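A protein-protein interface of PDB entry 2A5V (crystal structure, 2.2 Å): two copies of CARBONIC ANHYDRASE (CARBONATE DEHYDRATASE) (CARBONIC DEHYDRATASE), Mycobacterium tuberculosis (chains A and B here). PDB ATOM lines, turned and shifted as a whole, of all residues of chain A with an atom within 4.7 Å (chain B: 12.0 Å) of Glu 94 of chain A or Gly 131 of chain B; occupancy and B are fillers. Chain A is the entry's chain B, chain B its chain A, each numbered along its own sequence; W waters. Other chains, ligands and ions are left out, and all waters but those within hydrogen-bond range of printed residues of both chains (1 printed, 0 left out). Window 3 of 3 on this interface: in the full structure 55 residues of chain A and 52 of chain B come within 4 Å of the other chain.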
ATOM      1  N   LEU A  90      15.809  24.598  28.281  1.00  0.00           N
ATOM      2  CA  LEU A  90      16.020  25.589  27.264  1.00  0.00           C
ATOM      3  C   LEU A  90      14.742  25.918  26.477  1.00  0.00           C
ATOM      4  O   LEU A  90      14.456  27.089  26.215  1.00  0.00           O
ATOM      5  CB  LEU A  90      17.179  25.135  26.370  1.00  0.00           C
ATOM      6  CG  LEU A  90      17.987  26.190  25.629  1.00  0.00           C
ATOM      7  CD1 LEU A  90      18.097  27.517  26.374  1.00  0.00           C
ATOM      8  CD2 LEU A  90      19.344  25.599  25.327  1.00  0.00           C
ATOM      9  N   GLY A  91      13.951  24.906  26.101  1.00  0.00           N
ATOM     10  CA  GLY A  91      12.692  25.199  25.416  1.00  0.00           C
ATOM     11  C   GLY A  91      11.708  26.019  26.222  1.00  0.00           C
ATOM     12  O   GLY A  91      10.998  26.883  25.664  1.00  0.00           O
ATOM     13  N   SER A  92      11.649  25.744  27.526  1.00  0.00           N
ATOM     14  CA  SER A  92      10.828  26.513  28.489  1.00  0.00           C
ATOM     15  C   SER A  92      11.259  27.979  28.526  1.00  0.00           C
ATOM     16  O   SER A  92      10.425  28.886  28.512  1.00  0.00           O
ATOM     17  CB  SER A  92      10.914  25.909  29.916  1.00  0.00           C
ATOM     18  OG  SER A  92      10.540  24.501  29.955  1.00  0.00           O
ATOM     19  N   ILE A  93      12.556  28.240  28.627  1.00  0.00           N
ATOM     20  CA  ILE A  93      12.983  29.645  28.673  1.00  0.00           C
ATOM     21  C   ILE A  93      12.675  30.315  27.331  1.00  0.00           C
ATOM     22  O   ILE A  93      12.205  31.434  27.312  1.00  0.00           O
ATOM     23  CB  ILE A  93      14.491  29.800  29.054  1.00  0.00           C
ATOM     24  CG1 ILE A  93      14.736  29.306  30.497  1.00  0.00           C
ATOM     25  CG2 ILE A  93      14.931  31.283  28.909  1.00  0.00           C
ATOM     26  CD1 ILE A  93      16.072  28.863  30.800  1.00  0.00           C
ATOM     27  N   GLU A  94      12.952  29.603  26.224  1.00  0.00           N
ATOM     28  CA  GLU A  94      12.683  30.082  24.878  1.00  0.00           C
ATOM     29  C   GLU A  94      11.176  30.277  24.634  1.00  0.00           C
ATOM     30  O   GLU A  94      10.778  31.115  23.837  1.00  0.00           O
ATOM     31  CB  GLU A  94      13.275  29.113  23.817  1.00  0.00           C
ATOM     32  CG  GLU A  94      14.769  29.223  23.590  1.00  0.00           C
ATOM     33  CD  GLU A  94      15.219  28.730  22.220  1.00  0.00           C
ATOM     34  OE1 GLU A  94      16.387  28.993  21.862  1.00  0.00           O
ATOM     35  OE2 GLU A  94      14.431  28.098  21.473  1.00  0.00           O
ATOM     36  N   TYR A  95      10.331  29.478  25.273  1.00  0.00           N
ATOM     37  CA  TYR A  95       8.889  29.707  25.177  1.00  0.00           C
ATOM     38  C   TYR A  95       8.559  31.104  25.734  1.00  0.00           C
ATOM     39  O   TYR A  95       7.822  31.872  25.112  1.00  0.00           O
ATOM     40  CB  TYR A  95       8.110  28.610  25.907  1.00  0.00           C
ATOM     41  CG  TYR A  95       6.630  28.806  25.787  1.00  0.00           C
ATOM     42  CD1 TYR A  95       5.904  28.156  24.802  1.00  0.00           C
ATOM     43  CD2 TYR A  95       5.956  29.681  26.646  1.00  0.00           C
ATOM     44  CE1 TYR A  95       4.535  28.363  24.666  1.00  0.00           C
ATOM     45  CE2 TYR A  95       4.584  29.899  26.518  1.00  0.00           C
ATOM     46  CZ  TYR A  95       3.884  29.241  25.537  1.00  0.00           C
ATOM     47  OH  TYR A  95       2.540  29.463  25.437  1.00  0.00           O
ATOM     48  N   ALA A  96       9.132  31.448  26.887  1.00  0.00           N
ATOM     49  CA  ALA A  96       8.811  32.752  27.503  1.00  0.00           C
ATOM     50  C   ALA A  96       9.371  33.922  26.691  1.00  0.00           C
ATOM     51  O   ALA A  96       8.769  34.968  26.618  1.00  0.00           O
ATOM     52  CB  ALA A  96       9.348  32.813  28.940  1.00  0.00           C
ATOM     53  N   VAL A  97      10.544  33.711  26.103  1.00  0.00           N
ATOM     54  CA  VAL A  97      11.230  34.709  25.310  1.00  0.00           C
ATOM     55  C   VAL A  97      10.554  34.953  23.972  1.00  0.00           C
ATOM     56  O   VAL A  97      10.429  36.105  23.564  1.00  0.00           O
ATOM     57  CB  VAL A  97      12.700  34.290  25.096  1.00  0.00           C
ATOM     58  CG1 VAL A  97      13.335  35.082  24.018  1.00  0.00           C
ATOM     59  CG2 VAL A  97      13.464  34.466  26.409  1.00  0.00           C
ATOM     60  N   THR A  98      10.123  33.876  23.305  1.00  0.00           N
ATOM     61  CA  THR A  98       9.605  33.968  21.940  1.00  0.00           C
ATOM     62  C   THR A  98       8.079  33.970  21.819  1.00  0.00           C
ATOM     63  O   THR A  98       7.540  34.560  20.891  1.00  0.00           O
ATOM     64  CB  THR A  98      10.166  32.861  21.042  1.00  0.00           C
ATOM     65  OG1 THR A  98       9.591  31.613  21.431  1.00  0.00           O
ATOM     66  CG2 THR A  98      11.710  32.785  21.181  1.00  0.00           C
ATOM     67  N   VAL A  99       7.378  33.309  22.735  1.00  0.00           N
ATOM     68  CA  VAL A  99       5.898  33.263  22.665  1.00  0.00           C
ATOM     69  C   VAL A  99       5.323  34.324  23.585  1.00  0.00           C
ATOM     70  O   VAL A  99       4.367  35.011  23.242  1.00  0.00           O
ATOM     71  CB  VAL A  99       5.351  31.852  23.075  1.00  0.00           C
ATOM     72  CG1 VAL A  99       3.791  31.822  23.092  1.00  0.00           C
ATOM     73  CG2 VAL A  99       5.911  30.765  22.144  1.00  0.00           C
ATOM     74  N   SER A 174      21.180  29.513  22.431  1.00  0.00           N
ATOM     75  CA  SER A 174      19.902  30.004  21.971  1.00  0.00           C
ATOM     76  C   SER A 174      20.073  31.276  21.158  1.00  0.00           C
ATOM     77  O   SER A 174      20.342  32.345  21.704  1.00  0.00           O
ATOM     78  CB  SER A 174      18.959  30.229  23.147  1.00  0.00           C
ATOM     79  OG  SER A 174      17.744  30.769  22.691  1.00  0.00           O
ATOM     80  N   SER A 175      19.944  31.150  19.844  1.00  0.00           N
ATOM     81  CA  SER A 175      19.983  32.325  18.986  1.00  0.00           C
ATOM     82  C   SER A 175      18.725  33.170  19.169  1.00  0.00           C
ATOM     83  O   SER A 175      18.776  34.385  19.025  1.00  0.00           O
ATOM     84  CB  SER A 175      20.211  31.948  17.517  1.00  0.00           C
ATOM     85  OG  SER A 175      19.064  31.333  16.976  1.00  0.00           O
ATOM     86  N   ALA A 176      17.610  32.534  19.511  1.00  0.00           N
ATOM     87  CA  ALA A 176      16.397  33.251  19.888  1.00  0.00           C
ATOM     88  C   ALA A 176      16.679  34.280  20.999  1.00  0.00           C
ATOM     89  O   ALA A 176      16.221  35.425  20.938  1.00  0.00           O
ATOM     90  CB  ALA A 176      15.331  32.267  20.315  1.00  0.00           C
ATOM     91  N   ILE A 177      17.482  33.879  21.977  1.00  0.00           N
ATOM     92  CA  ILE A 177      17.861  34.744  23.097  1.00  0.00           C
ATOM     93  C   ILE A 177      18.907  35.776  22.697  1.00  0.00           C
ATOM     94  O   ILE A 177      18.719  36.965  22.911  1.00  0.00           O
ATOM     95  CB  ILE A 177      18.319  33.897  24.346  1.00  0.00           C
ATOM     96  CG1 ILE A 177      17.112  33.269  25.037  1.00  0.00           C
ATOM     97  CG2 ILE A 177      19.163  34.709  25.353  1.00  0.00           C
ATOM     98  CD1 ILE A 177      17.473  32.128  26.006  1.00  0.00           C
ATOM     99  N   ALA B  58       5.801  25.933  34.234  1.00  0.00           N
ATOM    100  CA  ALA B  58       6.434  27.257  34.329  1.00  0.00           C
ATOM    101  C   ALA B  58       5.463  28.439  34.179  1.00  0.00           C
ATOM    102  O   ALA B  58       5.803  29.576  34.473  1.00  0.00           O
ATOM    103  CB  ALA B  58       7.568  27.344  33.304  1.00  0.00           C
ATOM    104  N   ASP B  59       4.229  28.158  33.776  1.00  0.00           N
ATOM    105  CA  ASP B  59       3.226  29.181  33.585  1.00  0.00           C
ATOM    106  C   ASP B  59       3.220  30.155  34.788  1.00  0.00           C
ATOM    107  O   ASP B  59       3.181  29.727  35.944  1.00  0.00           O
ATOM    108  CB  ASP B  59       1.862  28.508  33.369  1.00  0.00           C
ATOM    109  CG  ASP B  59       0.757  29.487  32.959  1.00  0.00           C
ATOM    110  OD1 ASP B  59       0.426  30.407  33.721  1.00  0.00           O
ATOM    111  OD2 ASP B  59       0.216  29.328  31.855  1.00  0.00           O
ATOM    112  N   ARG B  79      10.039  23.257  37.770  1.00  0.00           N
ATOM    113  CA  ARG B  79       9.046  23.816  36.855  1.00  0.00           C
ATOM    114  C   ARG B  79       9.642  23.905  35.453  1.00  0.00           C
ATOM    115  O   ARG B  79      10.747  24.449  35.289  1.00  0.00           O
ATOM    116  CB  ARG B  79       8.593  25.198  37.337  1.00  0.00           C
ATOM    117  CG  ARG B  79       7.512  25.156  38.398  1.00  0.00           C
ATOM    118  CD  ARG B  79       7.294  26.492  39.098  1.00  0.00           C
ATOM    119  NE  ARG B  79       6.418  27.340  38.312  1.00  0.00           N
ATOM    120  CZ  ARG B  79       6.014  28.548  38.662  1.00  0.00           C
ATOM    121  NH1 ARG B  79       6.377  29.075  39.832  1.00  0.00           N
ATOM    122  NH2 ARG B  79       5.224  29.228  37.838  1.00  0.00           N
ATOM    123  N   THR B  80       8.928  23.312  34.479  1.00  0.00           N
ATOM    124  CA  THR B  80       9.215  23.447  33.033  1.00  0.00           C
ATOM    125  C   THR B  80       7.897  23.709  32.305  1.00  0.00           C
ATOM    126  O   THR B  80       6.811  23.494  32.872  1.00  0.00           O
ATOM    127  CB  THR B  80       9.899  22.188  32.397  1.00  0.00           C
ATOM    128  OG1 THR B  80       9.105  21.025  32.649  1.00  0.00           O
ATOM    129  CG2 THR B  80      11.315  21.967  32.956  1.00  0.00           C
ATOM    130  N   ALA B  81       7.980  24.184  31.064  1.00  0.00           N
ATOM    131  CA  ALA B  81       6.776  24.411  30.261  1.00  0.00           C
ATOM    132  C   ALA B  81       6.048  23.071  30.032  1.00  0.00           C
ATOM    133  O   ALA B  81       6.649  22.114  29.545  1.00  0.00           O
ATOM    134  CB  ALA B  81       7.125  25.083  28.944  1.00  0.00           C
ATOM    135  N   GLY B  82       4.781  23.011  30.434  1.00  0.00           N
ATOM    136  CA  GLY B  82       3.965  21.816  30.301  1.00  0.00           C
ATOM    137  C   GLY B  82       4.453  20.674  31.165  1.00  0.00           C
ATOM    138  O   GLY B  82       4.108  19.524  30.881  1.00  0.00           O
ATOM    139  N   VAL B  84       7.218  19.073  31.280  1.00  0.00           N
ATOM    140  CA  VAL B  84       7.921  18.054  30.524  1.00  0.00           C
ATOM    141  C   VAL B  84       9.261  17.684  31.186  1.00  0.00           C
ATOM    142  O   VAL B  84       9.917  18.488  31.877  1.00  0.00           O
ATOM    143  CB  VAL B  84       8.174  18.501  29.064  1.00  0.00           C
ATOM    144  CG1 VAL B  84       6.841  18.713  28.341  1.00  0.00           C
ATOM    145  CG2 VAL B  84       9.028  19.759  28.997  1.00  0.00           C
ATOM    146  N   ASP B  86      13.126  16.195  31.159  1.00  0.00           N
ATOM    147  CA  ASP B  86      14.401  15.892  30.522  1.00  0.00           C
ATOM    148  C   ASP B  86      15.269  15.404  31.666  1.00  0.00           C
ATOM    149  O   ASP B  86      14.781  15.256  32.794  1.00  0.00           O
ATOM    150  CB  ASP B  86      15.008  17.113  29.776  1.00  0.00           C
ATOM    151  CG  ASP B  86      15.401  18.321  30.721  1.00  0.00           C
ATOM    152  OD1 ASP B  86      15.718  18.143  31.927  1.00  0.00           O
ATOM    153  OD2 ASP B  86      15.427  19.493  30.246  1.00  0.00           O
ATOM    154  N   GLY B 114      -0.368  26.373  27.734  1.00  0.00           N
ATOM    155  CA  GLY B 114       0.086  26.663  26.379  1.00  0.00           C
ATOM    156  C   GLY B 114       0.910  25.554  25.733  1.00  0.00           C
ATOM    157  O   GLY B 114       0.965  25.480  24.515  1.00  0.00           O
ATOM    158  N   ALA B 115       1.573  24.722  26.543  1.00  0.00           N
ATOM    159  CA  ALA B 115       2.348  23.582  26.043  1.00  0.00           C
ATOM    160  C   ALA B 115       1.401  22.494  25.539  1.00  0.00           C
ATOM    161  O   ALA B 115       1.624  21.927  24.461  1.00  0.00           O
ATOM    162  CB  ALA B 115       3.286  23.033  27.122  1.00  0.00           C
ATOM    163  N   ALA B 118      -0.170  23.952  22.270  1.00  0.00           N
ATOM    164  CA  ALA B 118       0.794  23.840  21.158  1.00  0.00           C
ATOM    165  C   ALA B 118       0.904  22.422  20.574  1.00  0.00           C
ATOM    166  O   ALA B 118       1.037  22.240  19.362  1.00  0.00           O
ATOM    167  CB  ALA B 118       2.194  24.364  21.578  1.00  0.00           C
ATOM    168  N   THR B 127       1.124  22.679  12.896  1.00  0.00           N
ATOM    169  CA  THR B 127       1.764  23.905  13.382  1.00  0.00           C
ATOM    170  C   THR B 127       2.861  23.515  14.387  1.00  0.00           C
ATOM    171  O   THR B 127       2.555  23.058  15.492  1.00  0.00           O
ATOM    172  CB  THR B 127       0.757  24.843  14.101  1.00  0.00           C
ATOM    173  OG1 THR B 127      -0.450  24.964  13.347  1.00  0.00           O
ATOM    174  CG2 THR B 127       1.345  26.228  14.297  1.00  0.00           C
ATOM    175  N   LEU B 128       4.129  23.664  14.009  1.00  0.00           N
ATOM    176  CA  LEU B 128       5.219  23.376  14.942  1.00  0.00           C
ATOM    177  C   LEU B 128       6.058  24.611  15.206  1.00  0.00           C
ATOM    178  O   LEU B 128       6.358  25.366  14.279  1.00  0.00           O
ATOM    179  CB  LEU B 128       6.135  22.259  14.431  1.00  0.00           C
ATOM    180  CG  LEU B 128       5.755  20.776  14.596  1.00  0.00           C
ATOM    181  CD1 LEU B 128       6.562  19.987  13.618  1.00  0.00           C
ATOM    182  CD2 LEU B 128       5.958  20.215  16.022  1.00  0.00           C
ATOM    183  N   PRO B 129       6.474  24.804  16.462  1.00  0.00           N
ATOM    184  CA  PRO B 129       7.370  25.925  16.729  1.00  0.00           C
ATOM    185  C   PRO B 129       8.813  25.549  16.397  1.00  0.00           C
ATOM    186  O   PRO B 129       9.081  24.401  16.063  1.00  0.00           O
ATOM    187  CB  PRO B 129       7.150  26.186  18.219  1.00  0.00           C
ATOM    188  CG  PRO B 129       6.855  24.816  18.777  1.00  0.00           C
ATOM    189  CD  PRO B 129       6.189  24.018  17.680  1.00  0.00           C
ATOM    190  N   GLY B 130       9.729  26.509  16.443  1.00  0.00           N
ATOM    191  CA  GLY B 130      11.129  26.242  16.118  1.00  0.00           C
ATOM    192  C   GLY B 130      12.010  26.272  17.357  1.00  0.00           C
ATOM    193  O   GLY B 130      11.507  26.356  18.471  1.00  0.00           O
ATOM    194  N   GLY B 131      13.325  26.201  17.147  1.00  0.00           N
ATOM    195  CA  GLY B 131      14.288  26.141  18.222  1.00  0.00           C
ATOM    196  C   GLY B 131      13.939  25.068  19.236  1.00  0.00           C
ATOM    197  O   GLY B 131      13.424  23.994  18.884  1.00  0.00           O
ATOM    198  N   TYR B 132      14.205  25.371  20.498  1.00  0.00           N
ATOM    199  CA  TYR B 132      13.973  24.427  21.572  1.00  0.00           C
ATOM    200  C   TYR B 132      12.554  24.383  22.039  1.00  0.00           C
ATOM    201  O   TYR B 132      12.216  23.490  22.805  1.00  0.00           O
ATOM    202  CB  TYR B 132      14.872  24.710  22.771  1.00  0.00           C
ATOM    203  CG  TYR B 132      16.284  24.336  22.523  1.00  0.00           C
ATOM    204  CD1 TYR B 132      16.760  23.076  22.883  1.00  0.00           C
ATOM    205  CD2 TYR B 132      17.147  25.234  21.908  1.00  0.00           C
ATOM    206  CE1 TYR B 132      18.078  22.728  22.647  1.00  0.00           C
ATOM    207  CE2 TYR B 132      18.448  24.895  21.649  1.00  0.00           C
ATOM    208  CZ  TYR B 132      18.908  23.649  22.033  1.00  0.00           C
ATOM    209  OH  TYR B 132      20.217  23.337  21.773  1.00  0.00           O
ATOM    210  N   VAL B 133      11.736  25.356  21.637  1.00  0.00           N
ATOM    211  CA  VAL B 133      10.321  25.268  21.943  1.00  0.00           C
ATOM    212  C   VAL B 133       9.773  23.973  21.298  1.00  0.00           C
ATOM    213  O   VAL B 133       8.917  23.316  21.838  1.00  0.00           O
ATOM    214  CB  VAL B 133       9.497  26.541  21.507  1.00  0.00           C
ATOM    215  CG1 VAL B 133       8.035  26.362  21.878  1.00  0.00           C
ATOM    216  CG2 VAL B 133      10.037  27.833  22.172  1.00  0.00           C
ATOM    217  N   ARG B 134      10.281  23.602  20.137  1.00  0.00           N
ATOM    218  CA  ARG B 134       9.850  22.352  19.548  1.00  0.00           C
ATOM    219  C   ARG B 134      10.121  21.160  20.474  1.00  0.00           C
ATOM    220  O   ARG B 134       9.351  20.207  20.498  1.00  0.00           O
ATOM    221  CB  ARG B 134      10.547  22.125  18.208  1.00  0.00           C
ATOM    222  CG  ARG B 134      10.120  20.831  17.575  1.00  0.00           C
ATOM    223  CD  ARG B 134      10.680  20.663  16.193  1.00  0.00           C
ATOM    224  NE  ARG B 134      10.155  21.632  15.252  1.00  0.00           N
ATOM    225  CZ  ARG B 134      10.537  21.701  13.975  1.00  0.00           C
ATOM    226  NH1 ARG B 134      11.429  20.825  13.488  1.00  0.00           N
ATOM    227  NH2 ARG B 134      10.013  22.631  13.176  1.00  0.00           N
ATOM    228  N   ASP B 135      11.241  21.198  21.198  1.00  0.00           N
ATOM    229  CA  ASP B 135      11.580  20.128  22.146  1.00  0.00           C
ATOM    230  C   ASP B 135      10.535  19.989  23.229  1.00  0.00           C
ATOM    231  O   ASP B 135      10.204  18.859  23.607  1.00  0.00           O
ATOM    232  CB  ASP B 135      12.948  20.334  22.763  1.00  0.00           C
ATOM    233  CG  ASP B 135      14.056  20.265  21.712  1.00  0.00           C
ATOM    234  OD1 ASP B 135      15.082  19.580  21.924  1.00  0.00           O
ATOM    235  OD2 ASP B 135      13.879  20.876  20.640  1.00  0.00           O
ATOM    236  N   VAL B 136      10.012  21.113  23.721  1.00  0.00           N
ATOM    237  CA  VAL B 136       8.889  21.059  24.651  1.00  0.00           C
ATOM    238  C   VAL B 136       7.641  20.414  24.034  1.00  0.00           C
ATOM    239  O   VAL B 136       7.053  19.527  24.616  1.00  0.00           O
ATOM    240  CB  VAL B 136       8.568  22.444  25.220  1.00  0.00           C
ATOM    241  CG1 VAL B 136       7.252  22.408  25.994  1.00  0.00           C
ATOM    242  CG2 VAL B 136       9.735  22.925  26.105  1.00  0.00           C
ATOM    243  N   VAL B 137       7.254  20.844  22.841  1.00  0.00           N
ATOM    244  CA  VAL B 137       6.050  20.327  22.169  1.00  0.00           C
ATOM    245  C   VAL B 137       6.202  18.838  21.830  1.00  0.00           C
ATOM    246  O   VAL B 137       5.254  18.072  21.941  1.00  0.00           O
ATOM    247  CB  VAL B 137       5.724  21.191  20.909  1.00  0.00           C
ATOM    248  CG1 VAL B 137       4.586  20.604  20.105  1.00  0.00           C
ATOM    249  CG2 VAL B 137       5.374  22.620  21.352  1.00  0.00           C
ATOM    250  N   GLU B 138       7.408  18.432  21.437  1.00  0.00           N
ATOM    251  CA  GLU B 138       7.717  17.033  21.157  1.00  0.00           C
ATOM    252  C   GLU B 138       7.349  16.105  22.298  1.00  0.00           C
ATOM    253  O   GLU B 138       6.888  14.982  22.069  1.00  0.00           O
ATOM    254  CB  GLU B 138       9.218  16.872  20.903  1.00  0.00           C
ATOM    255  CG  GLU B 138       9.544  17.066  19.458  1.00  0.00           C
ATOM    256  CD  GLU B 138      11.021  17.192  19.189  1.00  0.00           C
ATOM    257  OE1 GLU B 138      11.857  16.811  20.055  1.00  0.00           O
ATOM    258  OE2 GLU B 138      11.328  17.677  18.082  1.00  0.00           O
ATOM    259  N   ARG B 139       7.592  16.581  23.512  1.00  0.00           N
ATOM    260  CA  ARG B 139       7.429  15.796  24.725  1.00  0.00           C
ATOM    261  C   ARG B 139       5.980  15.777  25.202  1.00  0.00           C
ATOM    262  O   ARG B 139       5.587  14.888  25.950  1.00  0.00           O
ATOM    263  CB  ARG B 139       8.343  16.353  25.827  1.00  0.00           C
ATOM    264  CG  ARG B 139       9.813  15.950  25.652  1.00  0.00           C
ATOM    265  CD  ARG B 139      10.689  16.706  26.609  1.00  0.00           C
ATOM    266  NE  ARG B 139      12.059  16.163  26.606  1.00  0.00           N
ATOM    267  CZ  ARG B 139      13.017  16.552  25.771  1.00  0.00           C
ATOM    268  NH1 ARG B 139      12.775  17.500  24.867  1.00  0.00           N
ATOM    269  NH2 ARG B 139      14.209  15.991  25.830  1.00  0.00           N
HETATM  270  O   HOH W   1       1.397  28.167  22.561  1.00  0.00           O
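N of Ala 81 of chain B sits at hydrogen-bond distance from OG of Ser 92 of chain A, 2.8 Å away. The side-chain carboxylate (OE2) of Glu 94 of chain A lies within hydrogen-bond range of the backbone NH (N) of Tyr 132 of chain B (2.9 Å).
The backbone carbonyl oxygen of Thr 80 of chain B sits at hydrogen-bond distance from the backbone NH of Ala 58 of chain B (3.0 Å). O of Val 84 of chain B lies within hydrogen-bond range of OG1 of Thr 80 of chain B. The backbone carbonyl oxygen of Glu 94 of chain A sits at hydrogen-bond distance from the side-chain hydroxyl of Thr 98 of chain A, 2.7 Å away.
Tyr 132 of chain B touches Leu 90 of chain A (CE2 to CD2, 3.9 Å). Tyr 132 of chain B touches Gly 91 of chain A. Val 133 of chain B touches Gly 91 of chain A (CG2 to O, 3.7 Å). Gly 91 of chain A touches Val 136 of chain B (C to CG2, 3.7 Å). CB of Thr 80 of chain B touches OG of Ser 92 of chain A, 3.4 Å away. N of Ser 92 of chain A touches CG2 of Val 136 of chain B, 3.7 Å away. Val 133 of chain B touches Glu 94 of chain A. Gly 114 of chain B touches Tyr 95 of chain A (CA to OH, 3.8 Å). Tyr 95 of chain A touches Val 133 of chain B. Val 133 of chain B touches Thr 98 of chain A (CG2 to OG1, 3.9 Å).
Gly 91 of chain A touches just these residues of chain B: Tyr 132 (3.2 Å), Val 133 (3.7 Å) and Val 136 (3.7 Å). Ser 92 of chain A touches just these residues of chain B: Thr 80, Ala 81 and Val 136. Glu 94 of chain A touches just these residues of chain B: Gly 131, Tyr 132 and Val 133. Of the printed residues of chain B, Tyr 95 of chain A touches Gly 114 and Val 133. No residue of chain B comes within 4 Å of Ala 96 of chain A. Of chain B, only Val 133 (3.9 Å) comes within 4 Å of Thr 98 of chain A. No residue of chain B comes within 4 Å of Val 99 of chain A. No residue of chain B comes within 4 Å of Ser 174 of chain A. Ser 175 of chain A touches none of the printed residues of chain B. No residue of chain B comes within 4 Å of Ala 176 of chain A. Of the printed residues of chain A, Thr 80 of chain B touches Ser 92 (3.4 Å). Of the printed residues of chain A, Gly 114 of chain B touches Tyr 95 (3.8 Å). Of chain A, only Glu 94 (3.8 Å) comes within 4 Å of Gly 131 of chain B. Of the printed residues of chain A, Val 133 of chain B touches Gly 91, Glu 94, Tyr 95 and Thr 98. Of the printed residues of chain A, Val 136 of chain B touches Gly 91 and Ser 92. The nearest residue of chain B that does not touch Glu 94 of chain A is Gly 130 of chain B (4.5 Å). The nearest printed residue of chain A that does not touch Gly 131 of chain B is Gly 91 of chain A (6.3 Å). The nearest printed residue of chain A that does not touch Val 136 of chain B is Leu 90 of chain A (5.8 Å).
Printed residues of chain A that touch a printed residue of chain B: Leu 90, Gly 91, Ser 92, Glu 94, Tyr 95 and Thr 98. Among the printed residues, no Asp or Glu carboxylate lies within 4 Å of a Lys or Arg side-chain nitrogen of the other chain.
No position is printed for both chains.
Water W1 bridges O of Gly 114 of chain B and OH of Tyr 95 of chain A.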
